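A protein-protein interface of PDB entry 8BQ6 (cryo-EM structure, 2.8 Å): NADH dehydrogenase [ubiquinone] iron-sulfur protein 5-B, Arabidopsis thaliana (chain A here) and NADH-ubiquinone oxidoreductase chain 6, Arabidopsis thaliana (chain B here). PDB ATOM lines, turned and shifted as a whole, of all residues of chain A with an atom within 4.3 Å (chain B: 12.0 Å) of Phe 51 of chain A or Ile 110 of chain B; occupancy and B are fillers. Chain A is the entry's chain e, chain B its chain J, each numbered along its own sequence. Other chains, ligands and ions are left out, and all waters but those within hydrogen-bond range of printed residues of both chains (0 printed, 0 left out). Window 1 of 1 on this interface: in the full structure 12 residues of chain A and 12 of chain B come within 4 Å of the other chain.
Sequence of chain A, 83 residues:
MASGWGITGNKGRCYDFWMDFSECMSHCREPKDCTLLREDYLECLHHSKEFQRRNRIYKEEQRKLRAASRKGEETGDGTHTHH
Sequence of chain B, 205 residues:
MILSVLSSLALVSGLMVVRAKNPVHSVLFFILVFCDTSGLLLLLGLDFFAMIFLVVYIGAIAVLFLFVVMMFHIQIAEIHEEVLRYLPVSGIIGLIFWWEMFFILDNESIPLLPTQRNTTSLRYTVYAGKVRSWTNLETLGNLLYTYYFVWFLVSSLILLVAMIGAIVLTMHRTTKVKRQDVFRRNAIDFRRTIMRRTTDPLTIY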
ATOM      1  N   HIS A  47      26.286  16.002  26.136  1.00  0.00           N
ATOM      2  CA  HIS A  47      26.881  17.311  26.433  1.00  0.00           C
ATOM      3  C   HIS A  47      26.596  17.751  27.862  1.00  0.00           C
ATOM      4  O   HIS A  47      26.304  18.922  28.113  1.00  0.00           O
ATOM      5  CB  HIS A  47      26.402  18.398  25.469  1.00  0.00           C
ATOM      6  CG  HIS A  47      26.285  17.949  24.049  1.00  0.00           C
ATOM      7  ND1 HIS A  47      27.381  17.719  23.249  1.00  0.00           N
ATOM      8  CD2 HIS A  47      25.199  17.693  23.284  1.00  0.00           C
ATOM      9  CE1 HIS A  47      26.976  17.339  22.051  1.00  0.00           C
ATOM     10  NE2 HIS A  47      25.656  17.314  22.046  1.00  0.00           N
ATOM     11  N   SER A  48      26.656  16.818  28.808  1.00  0.00           N
ATOM     12  CA  SER A  48      26.298  17.143  30.182  1.00  0.00           C
ATOM     13  C   SER A  48      27.325  18.070  30.822  1.00  0.00           C
ATOM     14  O   SER A  48      26.970  19.094  31.417  1.00  0.00           O
ATOM     15  CB  SER A  48      26.154  15.859  30.991  1.00  0.00           C
ATOM     16  OG  SER A  48      25.075  15.076  30.522  1.00  0.00           O
ATOM     17  N   LYS A  49      28.609  17.728  30.706  1.00  0.00           N
ATOM     18  CA  LYS A  49      29.638  18.494  31.400  1.00  0.00           C
ATOM     19  C   LYS A  49      29.854  19.853  30.747  1.00  0.00           C
ATOM     20  O   LYS A  49      30.090  20.851  31.439  1.00  0.00           O
ATOM     21  CB  LYS A  49      30.940  17.700  31.443  1.00  0.00           C
ATOM     22  CG  LYS A  49      30.886  16.507  32.374  1.00  0.00           C
ATOM     23  CD  LYS A  49      32.190  15.732  32.378  1.00  0.00           C
ATOM     24  CE  LYS A  49      32.767  15.600  30.988  1.00  0.00           C
ATOM     25  NZ  LYS A  49      32.216  14.403  30.317  1.00  0.00           N
ATOM     26  N   GLU A  50      29.765  19.909  29.417  1.00  0.00           N
ATOM     27  CA  GLU A  50      29.863  21.180  28.706  1.00  0.00           C
ATOM     28  C   GLU A  50      28.766  22.143  29.146  1.00  0.00           C
ATOM     29  O   GLU A  50      29.027  23.319  29.437  1.00  0.00           O
ATOM     30  CB  GLU A  50      29.776  20.931  27.202  1.00  0.00           C
ATOM     31  CG  GLU A  50      30.491  21.954  26.348  1.00  0.00           C
ATOM     32  CD  GLU A  50      30.046  21.910  24.897  1.00  0.00           C
ATOM     33  OE1 GLU A  50      30.260  20.874  24.232  1.00  0.00           O
ATOM     34  OE2 GLU A  50      29.486  22.915  24.419  1.00  0.00           O
ATOM     35  N   PHE A  51      27.523  21.658  29.186  1.00  0.00           N
ATOM     36  CA  PHE A  51      26.410  22.522  29.558  1.00  0.00           C
ATOM     37  C   PHE A  51      26.474  22.893  31.031  1.00  0.00           C
ATOM     38  O   PHE A  51      26.117  24.012  31.407  1.00  0.00           O
ATOM     39  CB  PHE A  51      25.081  21.849  29.227  1.00  0.00           C
ATOM     40  CG  PHE A  51      24.806  21.749  27.759  1.00  0.00           C
ATOM     41  CD1 PHE A  51      25.592  22.429  26.847  1.00  0.00           C
ATOM     42  CD2 PHE A  51      23.760  20.981  27.289  1.00  0.00           C
ATOM     43  CE1 PHE A  51      25.344  22.339  25.504  1.00  0.00           C
ATOM     44  CE2 PHE A  51      23.506  20.888  25.943  1.00  0.00           C
ATOM     45  CZ  PHE A  51      24.299  21.566  25.049  1.00  0.00           C
ATOM     46  N   GLN A  52      26.935  21.973  31.876  1.00  0.00           N
ATOM     47  CA  GLN A  52      27.127  22.301  33.283  1.00  0.00           C
ATOM     48  C   GLN A  52      28.141  23.428  33.453  1.00  0.00           C
ATOM     49  O   GLN A  52      27.920  24.365  34.228  1.00  0.00           O
ATOM     50  CB  GLN A  52      27.570  21.057  34.042  1.00  0.00           C
ATOM     51  CG  GLN A  52      26.696  20.718  35.220  1.00  0.00           C
ATOM     52  CD  GLN A  52      27.127  19.440  35.895  1.00  0.00           C
ATOM     53  OE1 GLN A  52      27.490  18.468  35.231  1.00  0.00           O
ATOM     54  NE2 GLN A  52      27.091  19.427  37.221  1.00  0.00           N
ATOM     55  N   ARG A  53      29.258  23.357  32.725  1.00  0.00           N
ATOM     56  CA  ARG A  53      30.264  24.411  32.810  1.00  0.00           C
ATOM     57  C   ARG A  53      29.728  25.750  32.300  1.00  0.00           C
ATOM     58  O   ARG A  53      29.967  26.806  32.912  1.00  0.00           O
ATOM     59  CB  ARG A  53      31.501  23.988  32.025  1.00  0.00           C
ATOM     60  CG  ARG A  53      32.374  25.131  31.590  1.00  0.00           C
ATOM     61  CD  ARG A  53      33.139  24.770  30.333  1.00  0.00           C
ATOM     62  NE  ARG A  53      34.343  25.574  30.166  1.00  0.00           N
ATOM     63  CZ  ARG A  53      35.367  25.578  31.009  1.00  0.00           C
ATOM     64  NH1 ARG A  53      35.368  24.835  32.105  1.00  0.00           N
ATOM     65  NH2 ARG A  53      36.425  26.335  30.740  1.00  0.00           N
ATOM     66  N   ARG A  54      29.003  25.732  31.180  1.00  0.00           N
ATOM     67  CA  ARG A  54      28.435  26.980  30.678  1.00  0.00           C
ATOM     68  C   ARG A  54      27.387  27.543  31.630  1.00  0.00           C
ATOM     69  O   ARG A  54      27.242  28.767  31.749  1.00  0.00           O
ATOM     70  CB  ARG A  54      27.846  26.775  29.289  1.00  0.00           C
ATOM     71  CG  ARG A  54      28.894  26.821  28.207  1.00  0.00           C
ATOM     72  CD  ARG A  54      28.483  26.013  27.009  1.00  0.00           C
ATOM     73  NE  ARG A  54      27.749  26.813  26.039  1.00  0.00           N
ATOM     74  CZ  ARG A  54      27.393  26.376  24.841  1.00  0.00           C
ATOM     75  NH1 ARG A  54      27.690  25.152  24.440  1.00  0.00           N
ATOM     76  NH2 ARG A  54      26.727  27.186  24.025  1.00  0.00           N
ATOM     77  N   ASN A  55      26.659  26.672  32.327  1.00  0.00           N
ATOM     78  CA  ASN A  55      25.717  27.154  33.324  1.00  0.00           C
ATOM     79  C   ASN A  55      26.439  27.754  34.517  1.00  0.00           C
ATOM     80  O   ASN A  55      25.945  28.714  35.111  1.00  0.00           O
ATOM     81  CB  ASN A  55      24.789  26.027  33.763  1.00  0.00           C
ATOM     82  CG  ASN A  55      23.812  25.630  32.677  1.00  0.00           C
ATOM     83  OD1 ASN A  55      23.651  26.335  31.682  1.00  0.00           O
ATOM     84  ND2 ASN A  55      23.135  24.510  32.875  1.00  0.00           N
ATOM     85  N   PHE B 102       9.237  12.806  34.186  1.00  0.00           N
ATOM     86  CA  PHE B 102       9.388  14.091  33.522  1.00  0.00           C
ATOM     87  C   PHE B 102      10.772  14.675  33.750  1.00  0.00           C
ATOM     88  O   PHE B 102      11.145  15.644  33.081  1.00  0.00           O
ATOM     89  CB  PHE B 102       8.333  15.087  34.010  1.00  0.00           C
ATOM     90  CG  PHE B 102       6.959  14.818  33.484  1.00  0.00           C
ATOM     91  CD1 PHE B 102       6.369  13.580  33.647  1.00  0.00           C
ATOM     92  CD2 PHE B 102       6.257  15.803  32.815  1.00  0.00           C
ATOM     93  CE1 PHE B 102       5.110  13.333  33.170  1.00  0.00           C
ATOM     94  CE2 PHE B 102       4.997  15.555  32.330  1.00  0.00           C
ATOM     95  CZ  PHE B 102       4.424  14.319  32.508  1.00  0.00           C
ATOM     96  N   PHE B 103      11.538  14.095  34.672  1.00  0.00           N
ATOM     97  CA  PHE B 103      12.852  14.597  35.052  1.00  0.00           C
ATOM     98  C   PHE B 103      13.924  13.522  34.986  1.00  0.00           C
ATOM     99  O   PHE B 103      14.906  13.592  35.734  1.00  0.00           O
ATOM    100  CB  PHE B 103      12.787  15.192  36.458  1.00  0.00           C
ATOM    101  CG  PHE B 103      11.541  15.975  36.714  1.00  0.00           C
ATOM    102  CD1 PHE B 103      10.565  15.494  37.566  1.00  0.00           C
ATOM    103  CD2 PHE B 103      11.343  17.197  36.098  1.00  0.00           C
ATOM    104  CE1 PHE B 103       9.413  16.218  37.793  1.00  0.00           C
ATOM    105  CE2 PHE B 103      10.198  17.926  36.325  1.00  0.00           C
ATOM    106  CZ  PHE B 103       9.231  17.437  37.172  1.00  0.00           C
ATOM    107  N   ILE B 104      13.722  12.538  34.097  1.00  0.00           N
ATOM    108  CA  ILE B 104      14.679  11.391  33.972  1.00  0.00           C
ATOM    109  C   ILE B 104      15.911  11.854  33.188  1.00  0.00           C
ATOM    110  O   ILE B 104      17.023  11.406  33.519  1.00  0.00           O
ATOM    111  CB  ILE B 104      13.972  10.177  33.320  1.00  0.00           C
ATOM    112  CG1 ILE B 104      14.796   8.892  33.386  1.00  0.00           C
ATOM    113  CG2 ILE B 104      13.547  10.469  31.894  1.00  0.00           C
ATOM    114  CD1 ILE B 104      13.962   7.656  33.578  1.00  0.00           C
ATOM    115  N   LEU B 105      15.719  12.734  32.206  1.00  0.00           N
ATOM    116  CA  LEU B 105      16.824  13.239  31.404  1.00  0.00           C
ATOM    117  C   LEU B 105      17.629  14.317  32.122  1.00  0.00           C
ATOM    118  O   LEU B 105      18.771  14.572  31.726  1.00  0.00           O
ATOM    119  CB  LEU B 105      16.298  13.783  30.067  1.00  0.00           C
ATOM    120  CG  LEU B 105      15.445  12.880  29.158  1.00  0.00           C
ATOM    121  CD1 LEU B 105      15.318  13.462  27.758  1.00  0.00           C
ATOM    122  CD2 LEU B 105      16.012  11.474  29.076  1.00  0.00           C
ATOM    123  N   ASP B 106      17.083  14.921  33.186  1.00  0.00           N
ATOM    124  CA  ASP B 106      17.678  16.134  33.745  1.00  0.00           C
ATOM    125  C   ASP B 106      19.095  15.887  34.253  1.00  0.00           C
ATOM    126  O   ASP B 106      19.988  16.715  34.044  1.00  0.00           O
ATOM    127  CB  ASP B 106      16.795  16.690  34.866  1.00  0.00           C
ATOM    128  CG  ASP B 106      15.493  17.286  34.349  1.00  0.00           C
ATOM    129  OD1 ASP B 106      14.951  16.770  33.350  1.00  0.00           O
ATOM    130  OD2 ASP B 106      15.016  18.282  34.928  1.00  0.00           O
ATOM    131  N   ASN B 107      19.319  14.757  34.928  1.00  0.00           N
ATOM    132  CA  ASN B 107      20.665  14.390  35.348  1.00  0.00           C
ATOM    133  C   ASN B 107      21.552  14.029  34.167  1.00  0.00           C
ATOM    134  O   ASN B 107      22.748  14.342  34.173  1.00  0.00           O
ATOM    135  CB  ASN B 107      20.613  13.210  36.318  1.00  0.00           C
ATOM    136  CG  ASN B 107      20.053  13.589  37.669  1.00  0.00           C
ATOM    137  OD1 ASN B 107      20.085  14.754  38.056  1.00  0.00           O
ATOM    138  ND2 ASN B 107      19.543  12.605  38.398  1.00  0.00           N
ATOM    139  N   GLU B 108      20.995  13.364  33.159  1.00  0.00           N
ATOM    140  CA  GLU B 108      21.817  12.920  32.044  1.00  0.00           C
ATOM    141  C   GLU B 108      21.941  13.995  30.974  1.00  0.00           C
ATOM    142  O   GLU B 108      23.031  14.210  30.433  1.00  0.00           O
ATOM    143  CB  GLU B 108      21.244  11.633  31.454  1.00  0.00           C
ATOM    144  CG  GLU B 108      22.178  10.950  30.487  1.00  0.00           C
ATOM    145  CD  GLU B 108      23.290  10.225  31.205  1.00  0.00           C
ATOM    146  OE1 GLU B 108      24.288  10.884  31.566  1.00  0.00           O
ATOM    147  OE2 GLU B 108      23.164   9.002  31.418  1.00  0.00           O
ATOM    148  N   SER B 109      20.850  14.685  30.664  1.00  0.00           N
ATOM    149  CA  SER B 109      20.836  15.723  29.638  1.00  0.00           C
ATOM    150  C   SER B 109      20.514  17.049  30.321  1.00  0.00           C
ATOM    151  O   SER B 109      19.355  17.461  30.406  1.00  0.00           O
ATOM    152  CB  SER B 109      19.831  15.397  28.547  1.00  0.00           C
ATOM    153  OG  SER B 109      18.516  15.384  29.070  1.00  0.00           O
ATOM    154  N   ILE B 110      21.552  17.713  30.803  1.00  0.00           N
ATOM    155  CA  ILE B 110      21.379  18.970  31.532  1.00  0.00           C
ATOM    156  C   ILE B 110      21.063  20.078  30.533  1.00  0.00           C
ATOM    157  O   ILE B 110      21.800  20.243  29.551  1.00  0.00           O
ATOM    158  CB  ILE B 110      22.631  19.293  32.332  1.00  0.00           C
ATOM    159  CG1 ILE B 110      22.792  18.280  33.462  1.00  0.00           C
ATOM    160  CG2 ILE B 110      22.552  20.695  32.896  1.00  0.00           C
ATOM    161  CD1 ILE B 110      24.182  18.220  34.007  1.00  0.00           C
ATOM    162  N   PRO B 111      19.988  20.832  30.732  1.00  0.00           N
ATOM    163  CA  PRO B 111      19.652  21.896  29.784  1.00  0.00           C
ATOM    164  C   PRO B 111      20.649  23.040  29.816  1.00  0.00           C
ATOM    165  O   PRO B 111      21.186  23.410  30.862  1.00  0.00           O
ATOM    166  CB  PRO B 111      18.268  22.357  30.248  1.00  0.00           C
ATOM    167  CG  PRO B 111      18.216  22.002  31.675  1.00  0.00           C
ATOM    168  CD  PRO B 111      19.023  20.751  31.839  1.00  0.00           C
ATOM    169  N   LEU B 112      20.874  23.613  28.640  1.00  0.00           N
ATOM    170  CA  LEU B 112      21.704  24.800  28.486  1.00  0.00           C
ATOM    171  C   LEU B 112      20.840  26.031  28.730  1.00  0.00           C
ATOM    172  O   LEU B 112      19.905  26.302  27.970  1.00  0.00           O
ATOM    173  CB  LEU B 112      22.321  24.835  27.094  1.00  0.00           C
ATOM    174  CG  LEU B 112      23.308  25.964  26.860  1.00  0.00           C
ATOM    175  CD1 LEU B 112      24.532  25.734  27.715  1.00  0.00           C
ATOM    176  CD2 LEU B 112      23.666  26.012  25.393  1.00  0.00           C
ATOM    177  N   LEU B 113      21.152  26.774  29.784  1.00  0.00           N
ATOM    178  CA  LEU B 113      20.366  27.954  30.124  1.00  0.00           C
ATOM    179  C   LEU B 113      20.650  29.081  29.136  1.00  0.00           C
ATOM    180  O   LEU B 113      21.813  29.312  28.784  1.00  0.00           O
ATOM    181  CB  LEU B 113      20.683  28.410  31.543  1.00  0.00           C
ATOM    182  CG  LEU B 113      20.332  27.443  32.672  1.00  0.00           C
ATOM    183  CD1 LEU B 113      21.022  27.883  33.940  1.00  0.00           C
ATOM    184  CD2 LEU B 113      18.828  27.357  32.881  1.00  0.00           C
ATOM    185  N   PRO B 114      19.628  29.804  28.676  1.00  0.00           N
ATOM    186  CA  PRO B 114      19.850  30.898  27.717  1.00  0.00           C
ATOM    187  C   PRO B 114      20.393  32.137  28.413  1.00  0.00           C
ATOM    188  O   PRO B 114      19.770  32.677  29.330  1.00  0.00           O
ATOM    189  CB  PRO B 114      18.455  31.146  27.134  1.00  0.00           C
ATOM    190  CG  PRO B 114      17.523  30.709  28.203  1.00  0.00           C
ATOM    191  CD  PRO B 114      18.203  29.623  28.996  1.00  0.00           C
ATOM    192  N   THR B 115      21.549  32.598  27.958  1.00  0.00           N
ATOM    193  CA  THR B 115      22.213  33.745  28.552  1.00  0.00           C
ATOM    194  C   THR B 115      21.916  35.007  27.751  1.00  0.00           C
ATOM    195  O   THR B 115      21.366  34.966  26.648  1.00  0.00           O
ATOM    196  CB  THR B 115      23.722  33.501  28.633  1.00  0.00           C
ATOM    197  OG1 THR B 115      24.315  33.722  27.348  1.00  0.00           O
ATOM    198  CG2 THR B 115      23.989  32.069  29.053  1.00  0.00           C
ATOM    199  N   THR B 119      25.038  33.616  21.548  1.00  0.00           N
ATOM    200  CA  THR B 119      25.774  32.380  21.321  1.00  0.00           C
ATOM    201  C   THR B 119      25.616  31.858  19.901  1.00  0.00           C
ATOM    202  O   THR B 119      26.266  30.868  19.550  1.00  0.00           O
ATOM    203  CB  THR B 119      25.330  31.299  22.313  1.00  0.00           C
ATOM    204  OG1 THR B 119      24.226  30.566  21.767  1.00  0.00           O
ATOM    205  CG2 THR B 119      24.910  31.924  23.637  1.00  0.00           C
ATOM    206  N   LEU B 122      28.771  31.454  17.700  1.00  0.00           N
ATOM    207  CA  LEU B 122      29.690  30.342  17.895  1.00  0.00           C
ATOM    208  C   LEU B 122      29.234  29.068  17.206  1.00  0.00           C
ATOM    209  O   LEU B 122      29.879  28.026  17.368  1.00  0.00           O
ATOM    210  CB  LEU B 122      29.893  30.071  19.382  1.00  0.00           C
ATOM    211  CG  LEU B 122      30.984  30.964  19.967  1.00  0.00           C
ATOM    212  CD1 LEU B 122      30.855  31.041  21.471  1.00  0.00           C
ATOM    213  CD2 LEU B 122      32.364  30.491  19.542  1.00  0.00           C
ATOM    214  N   ARG B 123      28.137  29.119  16.464  1.00  0.00           N
ATOM    215  CA  ARG B 123      27.764  28.006  15.607  1.00  0.00           C
ATOM    216  C   ARG B 123      28.815  27.840  14.517  1.00  0.00           C
ATOM    217  O   ARG B 123      29.031  28.748  13.710  1.00  0.00           O
ATOM    218  CB  ARG B 123      26.385  28.250  15.003  1.00  0.00           C
ATOM    219  CG  ARG B 123      25.483  27.036  15.025  1.00  0.00           C
ATOM    220  CD  ARG B 123      24.023  27.405  15.243  1.00  0.00           C
ATOM    221  NE  ARG B 123      23.729  27.782  16.620  1.00  0.00           N
ATOM    222  CZ  ARG B 123      22.564  28.269  17.027  1.00  0.00           C
ATOM    223  NH1 ARG B 123      21.567  28.470  16.180  1.00  0.00           N
ATOM    224  NH2 ARG B 123      22.392  28.554  18.315  1.00  0.00           N
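Printed residues of chain A that touch a printed residue of chain B: Ser 48, Phe 51, Gln 52, Arg 54 and Asn 55. Of the 17 printed residues of chain B, 5 touch a printed residue of chain A. Hydrophobic or aromatic side chains of chain B within 4 Å of the printed part of chain A: Ile 110, Leu 112 and Leu 113.
OD1 of Asn 55 of chain A is in hydrogen-bond range of N of Leu 113 of chain B, 3.2 Å away. The backbone carbonyl oxygen (O) of Glu 108 of chain B sits close to the side-chain hydroxyl (OG) of Ser 48 of chain A (2.2 Å). ND2 of Asn 55 of chain A is in hydrogen-bond range of O of Pro 111 of chain B, at 3.0 Å.
No residue of chain B comes within 4 Å of His 47 of chain A. No residue of chain B comes within 4 Å of Glu 50 of chain A. Phe 51 of chain A touches just these residues of chain B: Ile 110 and Leu 112. Of chain B, only Ile 110 comes within 4 Å of Gln 52 of chain A. Of chain B, only Leu 112 (3.6 Å) comes within 4 Å of Arg 54 of chain A. Leu 105 of chain B touches none of the printed residues of chain A. Of the printed residues of chain A, Glu 108 of chain B touches Ser 48. Of the printed residues of chain A, Pro 111 of chain B touches Asn 55 (3.0 Å). Printed residues of chain A within 4 Å of Leu 112 of chain B: Phe 51 (3.6 Å) and Arg 54 (3.6 Å). Of the printed residues of chain A, Leu 113 of chain B touches Asn 55 (3.2 Å). Thr 115 of chain B touches none of the printed residues of chain A. The nearest printed residue of chain A that does not touch Ile 110 of chain B is His 47 of chain A (4.9 Å).
Ser 48 of chain A touches Ile 110 of chain B (O to CD1, 3.9 Å). CD2 of Phe 51 of chain A touches O of Ile 110 of chain B, 3.1 Å away. CD1 of Phe 51 of chain A touches CD1 of Leu 112 of chain B (3.6 Å). OE1 of Gln 52 of chain A touches CD1 of Ile 110 of chain B, 3.5 Å away. Arg 54 of chain A touches Leu 112 of chain B. Asn 55 of chain A touches Ile 110 of chain B.
The backbone carbonyl oxygen (O) of Phe 51 of chain A sits close to the side-chain amide nitrogen (ND2) of Asn 55 of chain A, 3.4 Å away. The side-chain carboxylate (OE2) of Glu 50 of chain A is in salt-bridge range of the guanidinium group (NH1) of Arg 54 of chain A, at 2.9 Å.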
